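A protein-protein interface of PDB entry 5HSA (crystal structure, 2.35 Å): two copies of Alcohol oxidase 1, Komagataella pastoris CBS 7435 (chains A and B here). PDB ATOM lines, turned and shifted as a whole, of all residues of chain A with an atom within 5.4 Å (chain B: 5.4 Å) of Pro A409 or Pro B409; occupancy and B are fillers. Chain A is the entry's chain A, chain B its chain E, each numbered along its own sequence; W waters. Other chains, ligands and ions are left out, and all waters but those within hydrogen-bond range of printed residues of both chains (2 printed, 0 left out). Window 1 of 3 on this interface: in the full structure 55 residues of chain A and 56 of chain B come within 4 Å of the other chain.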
ATOM      1  N   ARG A 317     -29.103  -2.196   4.968  1.00  0.00           N
ATOM      2  CA  ARG A 317     -28.710  -3.511   4.490  1.00  0.00           C
ATOM      3  C   ARG A 317     -28.207  -3.420   3.044  1.00  0.00           C
ATOM      4  O   ARG A 317     -28.814  -2.726   2.230  1.00  0.00           O
ATOM      5  CB  ARG A 317     -29.919  -4.447   4.584  1.00  0.00           C
ATOM      6  CG  ARG A 317     -29.697  -5.721   5.345  1.00  0.00           C
ATOM      7  CD  ARG A 317     -29.871  -5.613   6.852  1.00  0.00           C
ATOM      8  NE  ARG A 317     -28.944  -6.563   7.450  1.00  0.00           N
ATOM      9  CZ  ARG A 317     -29.135  -7.252   8.567  1.00  0.00           C
ATOM     10  NH1 ARG A 317     -30.240  -7.125   9.279  1.00  0.00           N
ATOM     11  NH2 ARG A 317     -28.189  -8.080   8.968  1.00  0.00           N
ATOM     12  N   ARG A 330     -15.032  -5.736  11.829  1.00  0.00           N
ATOM     13  CA  ARG A 330     -15.502  -6.679  12.840  1.00  0.00           C
ATOM     14  C   ARG A 330     -14.357  -7.501  13.422  1.00  0.00           C
ATOM     15  O   ARG A 330     -14.426  -7.933  14.568  1.00  0.00           O
ATOM     16  CB  ARG A 330     -16.573  -7.618  12.264  1.00  0.00           C
ATOM     17  CG  ARG A 330     -17.956  -7.355  12.823  1.00  0.00           C
ATOM     18  CD  ARG A 330     -18.932  -8.464  12.478  1.00  0.00           C
ATOM     19  NE  ARG A 330     -19.040  -8.636  11.033  1.00  0.00           N
ATOM     20  CZ  ARG A 330     -19.987  -8.091  10.273  1.00  0.00           C
ATOM     21  NH1 ARG A 330     -19.984  -8.318   8.965  1.00  0.00           N
ATOM     22  NH2 ARG A 330     -20.937  -7.340  10.819  1.00  0.00           N
ATOM     23  N   HIS A 405     -20.096  -2.692  16.066  1.00  0.00           N
ATOM     24  CA  HIS A 405     -20.531  -3.910  15.392  1.00  0.00           C
ATOM     25  C   HIS A 405     -21.027  -5.001  16.340  1.00  0.00           C
ATOM     26  O   HIS A 405     -21.696  -5.937  15.896  1.00  0.00           O
ATOM     27  CB  HIS A 405     -19.401  -4.471  14.523  1.00  0.00           C
ATOM     28  CG  HIS A 405     -19.304  -3.818  13.178  1.00  0.00           C
ATOM     29  ND1 HIS A 405     -18.557  -2.685  12.957  1.00  0.00           N
ATOM     30  CD2 HIS A 405     -19.892  -4.128  11.996  1.00  0.00           C
ATOM     31  CE1 HIS A 405     -18.674  -2.330  11.686  1.00  0.00           C
ATOM     32  NE2 HIS A 405     -19.475  -3.189  11.084  1.00  0.00           N
ATOM     33  N   THR A 406     -20.717  -4.890  17.632  1.00  0.00           N
ATOM     34  CA  THR A 406     -21.215  -5.885  18.580  1.00  0.00           C
ATOM     35  C   THR A 406     -22.670  -5.612  18.950  1.00  0.00           C
ATOM     36  O   THR A 406     -23.276  -6.400  19.675  1.00  0.00           O
ATOM     37  CB  THR A 406     -20.373  -5.950  19.888  1.00  0.00           C
ATOM     38  OG1 THR A 406     -20.504  -4.730  20.626  1.00  0.00           O
ATOM     39  CG2 THR A 406     -18.915  -6.207  19.587  1.00  0.00           C
ATOM     40  N   LYS A 407     -23.230  -4.510  18.449  1.00  0.00           N
ATOM     41  CA  LYS A 407     -24.615  -4.132  18.754  1.00  0.00           C
ATOM     42  C   LYS A 407     -25.503  -4.076  17.509  1.00  0.00           C
ATOM     43  O   LYS A 407     -26.580  -3.483  17.536  1.00  0.00           O
ATOM     44  CB  LYS A 407     -24.668  -2.771  19.467  1.00  0.00           C
ATOM     45  CG  LYS A 407     -23.678  -2.577  20.605  1.00  0.00           C
ATOM     46  CD  LYS A 407     -23.920  -3.553  21.743  1.00  0.00           C
ATOM     47  CE  LYS A 407     -23.242  -3.081  23.032  1.00  0.00           C
ATOM     48  NZ  LYS A 407     -21.766  -2.935  22.879  1.00  0.00           N
ATOM     49  N   ILE A 408     -25.051  -4.687  16.417  1.00  0.00           N
ATOM     50  CA  ILE A 408     -25.825  -4.721  15.181  1.00  0.00           C
ATOM     51  C   ILE A 408     -25.706  -6.148  14.641  1.00  0.00           C
ATOM     52  O   ILE A 408     -24.720  -6.827  14.931  1.00  0.00           O
ATOM     53  CB  ILE A 408     -25.315  -3.648  14.160  1.00  0.00           C
ATOM     54  CG1 ILE A 408     -26.458  -3.090  13.301  1.00  0.00           C
ATOM     55  CG2 ILE A 408     -24.137  -4.173  13.318  1.00  0.00           C
ATOM     56  CD1 ILE A 408     -26.011  -2.048  12.280  1.00  0.00           C
ATOM     57  N   PRO A 409     -26.717  -6.633  13.899  1.00  0.00           N
ATOM     58  CA  PRO A 409     -26.635  -8.023  13.428  1.00  0.00           C
ATOM     59  C   PRO A 409     -25.466  -8.264  12.473  1.00  0.00           C
ATOM     60  O   PRO A 409     -24.904  -7.310  11.941  1.00  0.00           O
ATOM     61  CB  PRO A 409     -27.967  -8.225  12.706  1.00  0.00           C
ATOM     62  CG  PRO A 409     -28.885  -7.227  13.328  1.00  0.00           C
ATOM     63  CD  PRO A 409     -28.024  -6.032  13.589  1.00  0.00           C
ATOM     64  N   PRO A 410     -25.092  -9.532  12.266  1.00  0.00           N
ATOM     65  CA  PRO A 410     -24.072  -9.833  11.260  1.00  0.00           C
ATOM     66  C   PRO A 410     -24.539  -9.453   9.859  1.00  0.00           C
ATOM     67  O   PRO A 410     -25.733  -9.208   9.649  1.00  0.00           O
ATOM     68  CB  PRO A 410     -23.879 -11.348  11.386  1.00  0.00           C
ATOM     69  CG  PRO A 410     -25.090 -11.839  12.075  1.00  0.00           C
ATOM     70  CD  PRO A 410     -25.543 -10.741  12.977  1.00  0.00           C
ATOM     71  N   GLY A 411     -23.605  -9.400   8.915  1.00  0.00           N
ATOM     72  CA  GLY A 411     -23.922  -9.042   7.548  1.00  0.00           C
ATOM     73  C   GLY A 411     -23.190  -7.789   7.114  1.00  0.00           C
ATOM     74  O   GLY A 411     -22.329  -7.278   7.833  1.00  0.00           O
ATOM     75  N   TYR A 413     -23.306  -3.731   5.402  1.00  0.00           N
ATOM     76  CA  TYR A 413     -24.136  -2.538   5.482  1.00  0.00           C
ATOM     77  C   TYR A 413     -23.582  -1.377   4.663  1.00  0.00           C
ATOM     78  O   TYR A 413     -22.457  -1.422   4.174  1.00  0.00           O
ATOM     79  CB  TYR A 413     -24.278  -2.079   6.938  1.00  0.00           C
ATOM     80  CG  TYR A 413     -24.853  -3.106   7.881  1.00  0.00           C
ATOM     81  CD1 TYR A 413     -26.226  -3.254   8.019  1.00  0.00           C
ATOM     82  CD2 TYR A 413     -24.020  -3.926   8.643  1.00  0.00           C
ATOM     83  CE1 TYR A 413     -26.761  -4.198   8.880  1.00  0.00           C
ATOM     84  CE2 TYR A 413     -24.545  -4.868   9.511  1.00  0.00           C
ATOM     85  CZ  TYR A 413     -25.915  -4.997   9.625  1.00  0.00           C
ATOM     86  OH  TYR A 413     -26.441  -5.923  10.485  1.00  0.00           O
ATOM     87  N   VAL A 477     -32.223  -1.344   8.697  1.00  0.00           N
ATOM     88  CA  VAL A 477     -31.919  -1.918  10.001  1.00  0.00           C
ATOM     89  C   VAL A 477     -32.842  -1.329  11.057  1.00  0.00           C
ATOM     90  O   VAL A 477     -32.622  -0.210  11.528  1.00  0.00           O
ATOM     91  CB  VAL A 477     -30.453  -1.669  10.394  1.00  0.00           C
ATOM     92  CG1 VAL A 477     -30.101  -2.387  11.693  1.00  0.00           C
ATOM     93  CG2 VAL A 477     -29.522  -2.087   9.266  1.00  0.00           C
ATOM     94  N   SER A 479     -33.561  -1.652  14.223  1.00  0.00           N
ATOM     95  CA  SER A 479     -33.082  -1.219  15.532  1.00  0.00           C
ATOM     96  C   SER A 479     -32.355   0.121  15.490  1.00  0.00           C
ATOM     97  O   SER A 479     -32.229   0.788  16.523  1.00  0.00           O
ATOM     98  CB  SER A 479     -32.154  -2.268  16.126  1.00  0.00           C
ATOM     99  OG  SER A 479     -31.012  -2.453  15.313  1.00  0.00           O
ATOM    100  N   GLU A 494     -36.862  -4.748   6.864  1.00  0.00           N
ATOM    101  CA  GLU A 494     -35.611  -5.494   6.837  1.00  0.00           C
ATOM    102  C   GLU A 494     -35.415  -6.260   5.530  1.00  0.00           C
ATOM    103  O   GLU A 494     -36.302  -6.287   4.675  1.00  0.00           O
ATOM    104  CB  GLU A 494     -35.566  -6.467   8.019  1.00  0.00           C
ATOM    105  CG  GLU A 494     -34.747  -5.982   9.213  1.00  0.00           C
ATOM    106  CD  GLU A 494     -33.234  -6.177   9.027  1.00  0.00           C
ATOM    107  OE1 GLU A 494     -32.485  -6.000  10.012  1.00  0.00           O
ATOM    108  OE2 GLU A 494     -32.780  -6.514   7.907  1.00  0.00           O
ATOM    109  N   ARG B 317     -28.206 -10.991  27.201  1.00  0.00           N
ATOM    110  CA  ARG B 317     -26.791 -11.238  26.992  1.00  0.00           C
ATOM    111  C   ARG B 317     -26.263 -12.227  28.052  1.00  0.00           C
ATOM    112  O   ARG B 317     -26.620 -12.121  29.225  1.00  0.00           O
ATOM    113  CB  ARG B 317     -26.054  -9.900  27.071  1.00  0.00           C
ATOM    114  CG  ARG B 317     -25.166  -9.565  25.905  1.00  0.00           C
ATOM    115  CD  ARG B 317     -25.879  -8.910  24.738  1.00  0.00           C
ATOM    116  NE  ARG B 317     -25.206  -9.348  23.523  1.00  0.00           N
ATOM    117  CZ  ARG B 317     -25.040  -8.636  22.416  1.00  0.00           C
ATOM    118  NH1 ARG B 317     -25.500  -7.397  22.313  1.00  0.00           N
ATOM    119  NH2 ARG B 317     -24.399  -9.191  21.402  1.00  0.00           N
ATOM    120  N   ARG B 330     -26.821 -20.713  14.442  1.00  0.00           N
ATOM    121  CA  ARG B 330     -26.398 -19.704  13.472  1.00  0.00           C
ATOM    122  C   ARG B 330     -25.802 -20.363  12.241  1.00  0.00           C
ATOM    123  O   ARG B 330     -25.877 -19.816  11.144  1.00  0.00           O
ATOM    124  CB  ARG B 330     -25.386 -18.720  14.078  1.00  0.00           C
ATOM    125  CG  ARG B 330     -26.008 -17.369  14.423  1.00  0.00           C
ATOM    126  CD  ARG B 330     -24.969 -16.273  14.634  1.00  0.00           C
ATOM    127  NE  ARG B 330     -24.216 -16.485  15.865  1.00  0.00           N
ATOM    128  CZ  ARG B 330     -24.499 -15.915  17.033  1.00  0.00           C
ATOM    129  NH1 ARG B 330     -23.741 -16.183  18.087  1.00  0.00           N
ATOM    130  NH2 ARG B 330     -25.527 -15.080  17.146  1.00  0.00           N
ATOM    131  N   HIS B 405     -31.621 -15.256  13.981  1.00  0.00           N
ATOM    132  CA  HIS B 405     -30.272 -14.823  14.315  1.00  0.00           C
ATOM    133  C   HIS B 405     -29.690 -13.798  13.336  1.00  0.00           C
ATOM    134  O   HIS B 405     -28.710 -13.135  13.658  1.00  0.00           O
ATOM    135  CB  HIS B 405     -29.331 -16.022  14.401  1.00  0.00           C
ATOM    136  CG  HIS B 405     -29.376 -16.725  15.719  1.00  0.00           C
ATOM    137  ND1 HIS B 405     -30.277 -17.731  15.995  1.00  0.00           N
ATOM    138  CD2 HIS B 405     -28.636 -16.563  16.841  1.00  0.00           C
ATOM    139  CE1 HIS B 405     -30.092 -18.157  17.233  1.00  0.00           C
ATOM    140  NE2 HIS B 405     -29.098 -17.470  17.766  1.00  0.00           N
ATOM    141  N   THR B 406     -30.278 -13.662  12.151  1.00  0.00           N
ATOM    142  CA  THR B 406     -29.794 -12.670  11.199  1.00  0.00           C
ATOM    143  C   THR B 406     -30.267 -11.268  11.580  1.00  0.00           C
ATOM    144  O   THR B 406     -29.870 -10.286  10.945  1.00  0.00           O
ATOM    145  CB  THR B 406     -30.253 -12.977   9.754  1.00  0.00           C
ATOM    146  OG1 THR B 406     -31.679 -12.860   9.657  1.00  0.00           O
ATOM    147  CG2 THR B 406     -29.835 -14.367   9.338  1.00  0.00           C
ATOM    148  N   LYS B 407     -31.105 -11.177  12.616  1.00  0.00           N
ATOM    149  CA  LYS B 407     -31.682  -9.900  13.033  1.00  0.00           C
ATOM    150  C   LYS B 407     -31.300  -9.534  14.470  1.00  0.00           C
ATOM    151  O   LYS B 407     -31.925  -8.672  15.088  1.00  0.00           O
ATOM    152  CB  LYS B 407     -33.209  -9.924  12.917  1.00  0.00           C
ATOM    153  CG  LYS B 407     -33.773 -10.456  11.612  1.00  0.00           C
ATOM    154  CD  LYS B 407     -33.387  -9.599  10.428  1.00  0.00           C
ATOM    155  CE  LYS B 407     -34.299  -9.887   9.228  1.00  0.00           C
ATOM    156  NZ  LYS B 407     -34.240 -11.315   8.789  1.00  0.00           N
ATOM    157  N   ILE B 408     -30.285 -10.199  15.004  1.00  0.00           N
ATOM    158  CA  ILE B 408     -29.802  -9.910  16.348  1.00  0.00           C
ATOM    159  C   ILE B 408     -28.271  -9.891  16.269  1.00  0.00           C
ATOM    160  O   ILE B 408     -27.701 -10.529  15.378  1.00  0.00           O
ATOM    161  CB  ILE B 408     -30.333 -10.958  17.378  1.00  0.00           C
ATOM    162  CG1 ILE B 408     -30.550 -10.330  18.767  1.00  0.00           C
ATOM    163  CG2 ILE B 408     -29.450 -12.204  17.429  1.00  0.00           C
ATOM    164  CD1 ILE B 408     -31.069 -11.305  19.811  1.00  0.00           C
ATOM    165  N   PRO B 409     -27.595  -9.131  17.158  1.00  0.00           N
ATOM    166  CA  PRO B 409     -26.133  -9.054  17.023  1.00  0.00           C
ATOM    167  C   PRO B 409     -25.458 -10.395  17.267  1.00  0.00           C
ATOM    168  O   PRO B 409     -26.092 -11.294  17.813  1.00  0.00           O
ATOM    169  CB  PRO B 409     -25.732  -8.035  18.105  1.00  0.00           C
ATOM    170  CG  PRO B 409     -26.952  -7.215  18.305  1.00  0.00           C
ATOM    171  CD  PRO B 409     -28.094  -8.172  18.158  1.00  0.00           C
ATOM    172  N   PRO B 410     -24.184 -10.531  16.862  1.00  0.00           N
ATOM    173  CA  PRO B 410     -23.439 -11.750  17.197  1.00  0.00           C
ATOM    174  C   PRO B 410     -23.261 -11.888  18.707  1.00  0.00           C
ATOM    175  O   PRO B 410     -23.495 -10.932  19.443  1.00  0.00           O
ATOM    176  CB  PRO B 410     -22.092 -11.554  16.491  1.00  0.00           C
ATOM    177  CG  PRO B 410     -21.998 -10.098  16.229  1.00  0.00           C
ATOM    178  CD  PRO B 410     -23.387  -9.590  16.059  1.00  0.00           C
ATOM    179  N   GLY B 411     -22.858 -13.070  19.158  1.00  0.00           N
ATOM    180  CA  GLY B 411     -22.662 -13.313  20.574  1.00  0.00           C
ATOM    181  C   GLY B 411     -23.558 -14.428  21.070  1.00  0.00           C
ATOM    182  O   GLY B 411     -24.221 -15.105  20.277  1.00  0.00           O
ATOM    183  N   TYR B 413     -26.596 -15.809  23.977  1.00  0.00           N
ATOM    184  CA  TYR B 413     -27.780 -15.286  24.638  1.00  0.00           C
ATOM    185  C   TYR B 413     -28.480 -16.323  25.506  1.00  0.00           C
ATOM    186  O   TYR B 413     -28.174 -17.513  25.456  1.00  0.00           O
ATOM    187  CB  TYR B 413     -28.784 -14.767  23.605  1.00  0.00           C
ATOM    188  CG  TYR B 413     -28.260 -13.684  22.693  1.00  0.00           C
ATOM    189  CD1 TYR B 413     -28.265 -12.352  23.088  1.00  0.00           C
ATOM    190  CD2 TYR B 413     -27.767 -13.995  21.430  1.00  0.00           C
ATOM    191  CE1 TYR B 413     -27.791 -11.355  22.255  1.00  0.00           C
ATOM    192  CE2 TYR B 413     -27.293 -13.002  20.583  1.00  0.00           C
ATOM    193  CZ  TYR B 413     -27.312 -11.684  21.006  1.00  0.00           C
ATOM    194  OH  TYR B 413     -26.847 -10.699  20.182  1.00  0.00           O
ATOM    195  N   VAL B 477     -30.667  -7.053  25.587  1.00  0.00           N
ATOM    196  CA  VAL B 477     -30.659  -6.747  24.155  1.00  0.00           C
ATOM    197  C   VAL B 477     -31.696  -5.680  23.837  1.00  0.00           C
ATOM    198  O   VAL B 477     -32.882  -5.970  23.731  1.00  0.00           O
ATOM    199  CB  VAL B 477     -30.930  -8.021  23.321  1.00  0.00           C
ATOM    200  CG1 VAL B 477     -30.706  -7.770  21.842  1.00  0.00           C
ATOM    201  CG2 VAL B 477     -30.063  -9.168  23.815  1.00  0.00           C
ATOM    202  N   SER B 479     -32.739  -3.871  21.355  1.00  0.00           N
ATOM    203  CA  SER B 479     -33.617  -3.936  20.195  1.00  0.00           C
ATOM    204  C   SER B 479     -34.776  -4.903  20.393  1.00  0.00           C
ATOM    205  O   SER B 479     -35.794  -4.807  19.699  1.00  0.00           O
ATOM    206  CB  SER B 479     -32.823  -4.340  18.950  1.00  0.00           C
ATOM    207  OG  SER B 479     -32.245  -5.621  19.134  1.00  0.00           O
ATOM    208  N   GLU B 494     -27.150  -2.712  27.844  1.00  0.00           N
ATOM    209  CA  GLU B 494     -26.368  -3.701  27.106  1.00  0.00           C
ATOM    210  C   GLU B 494     -25.133  -4.161  27.873  1.00  0.00           C
ATOM    211  O   GLU B 494     -24.825  -3.636  28.938  1.00  0.00           O
ATOM    212  CB  GLU B 494     -25.944  -3.126  25.752  1.00  0.00           C
ATOM    213  CG  GLU B 494     -26.820  -3.542  24.590  1.00  0.00           C
ATOM    214  CD  GLU B 494     -26.507  -4.949  24.084  1.00  0.00           C
ATOM    215  OE1 GLU B 494     -27.049  -5.312  23.019  1.00  0.00           O
ATOM    216  OE2 GLU B 494     -25.722  -5.688  24.734  1.00  0.00           O
HETATM  217  O   HOH W   1     -27.552 -10.991   9.414  1.00  0.00           O
HETATM  218  O   HOH W   2     -21.918  -8.817  19.974  1.00  0.00           O
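The guanidinium group (NH2) of Arg A317 lies within hydrogen-bond range of the backbone carbonyl oxygen (O) of Thr B406.
O of Thr A406 lies within hydrogen-bond range of NH2 of Arg B317 (3.5 Å).
NH2 of Arg A317 sits at hydrogen-bond distance from OH of Tyr A413, 3.2 Å away.
OH of Tyr A413 sits at hydrogen-bond distance from O of Pro A409 (2.5 Å).
NH1 of Arg B317 lies within salt-bridge range of OE1 of Glu B494.
The side-chain hydroxyl (OG1) of Thr B406 sits at hydrogen-bond distance from the side-chain amino group (NZ) of Lys B407 (3.1 Å).
The backbone carbonyl oxygen of Pro B409 sits at hydrogen-bond distance from the side-chain hydroxyl of Tyr B413 (2.6 Å).
O of Pro A410 sits at hydrogen-bond distance from OH of Tyr A413 (3.5 Å).
O of Thr A406 touches CB of Pro B409, at 3.3 Å.
Glu B494 touches Lys A407.
CA of Pro B409 touches O of Ile A408 (3.4 Å).
CD of Pro B410 touches O of Ile A408 (3.3 Å).
Thr B406 touches Pro A409.
Pro B409 touches Pro A409.
Pro A410 touches Ile B408 (CD to O, 3.2 Å).
CD of Pro B410 touches CD of Pro A410 (3.9 Å).
Ser A479 touches Ser B479.
Glu A494 touches Lys B407.
Printed residues of chain B within 4 Å of Arg A317: Thr B406 (3.4 Å).
His A405 touches none of the printed residues of chain B.
Pro A409 touches just these residues of chain B: Thr B406 (3.3 Å), Lys B407 (3.5 Å), Ile B408 (3.3 Å) and Pro B409 (3.8 Å).
Of the printed residues of chain B, Pro A410 touches Ile B408 (3.2 Å) and Pro B410 (3.9 Å).
Pro B409 touches just these residues of chain A: Thr A406 (3.3 Å), Lys A407 (3.5 Å), Ile A408 (3.4 Å) and Pro A409 (3.8 Å).
Of the printed residues of chain A, Pro B410 touches Ile A408 (3.3 Å) and Pro A410 (3.9 Å).
Val B477 touches none of the printed residues of chain A.
The nearest residue of chain A that does not touch Pro B409 is Pro A410 (4.3 Å).
The nearest printed residue of chain A that does not touch Glu B494 is Thr A406 (5.2 Å).
Hydrophobic or aromatic side chains of chain B that line the printed part of chain A: Pro B409 and Pro B410.
Hydrophobic or aromatic side chains of chain A within 4 Å of the printed part of chain B: Pro A409 and Pro A410.
Among the printed residues, no Asp or Glu carboxylate lies within 4 Å of a Lys or Arg side-chain nitrogen of the other chain.
Thr A406 touches Pro B409, and with the chains exchanged Pro A409 touches Thr B406.
Ile A408 touches Pro B410, and with the chains exchanged Pro A410 touches Ile B408.
Pro A409 touches its own counterpart, Pro B409.
Ser A479 touches its own counterpart, Ser B479.
Of the 15 pairs that touch across the chains among the printed residues, 15 have their exchanged pair printed and touching as well.
Water W1 lies within hydrogen-bond range of O of Pro A410 (2.6 Å), O of Thr B406 (2.9 Å) and NH2 of Arg A317 (3.0 Å).
Water W2 lies within hydrogen-bond range of O of Pro B410 (2.7 Å), O of Thr A406 (2.8 Å) and NH2 of Arg B317 (2.9 Å).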
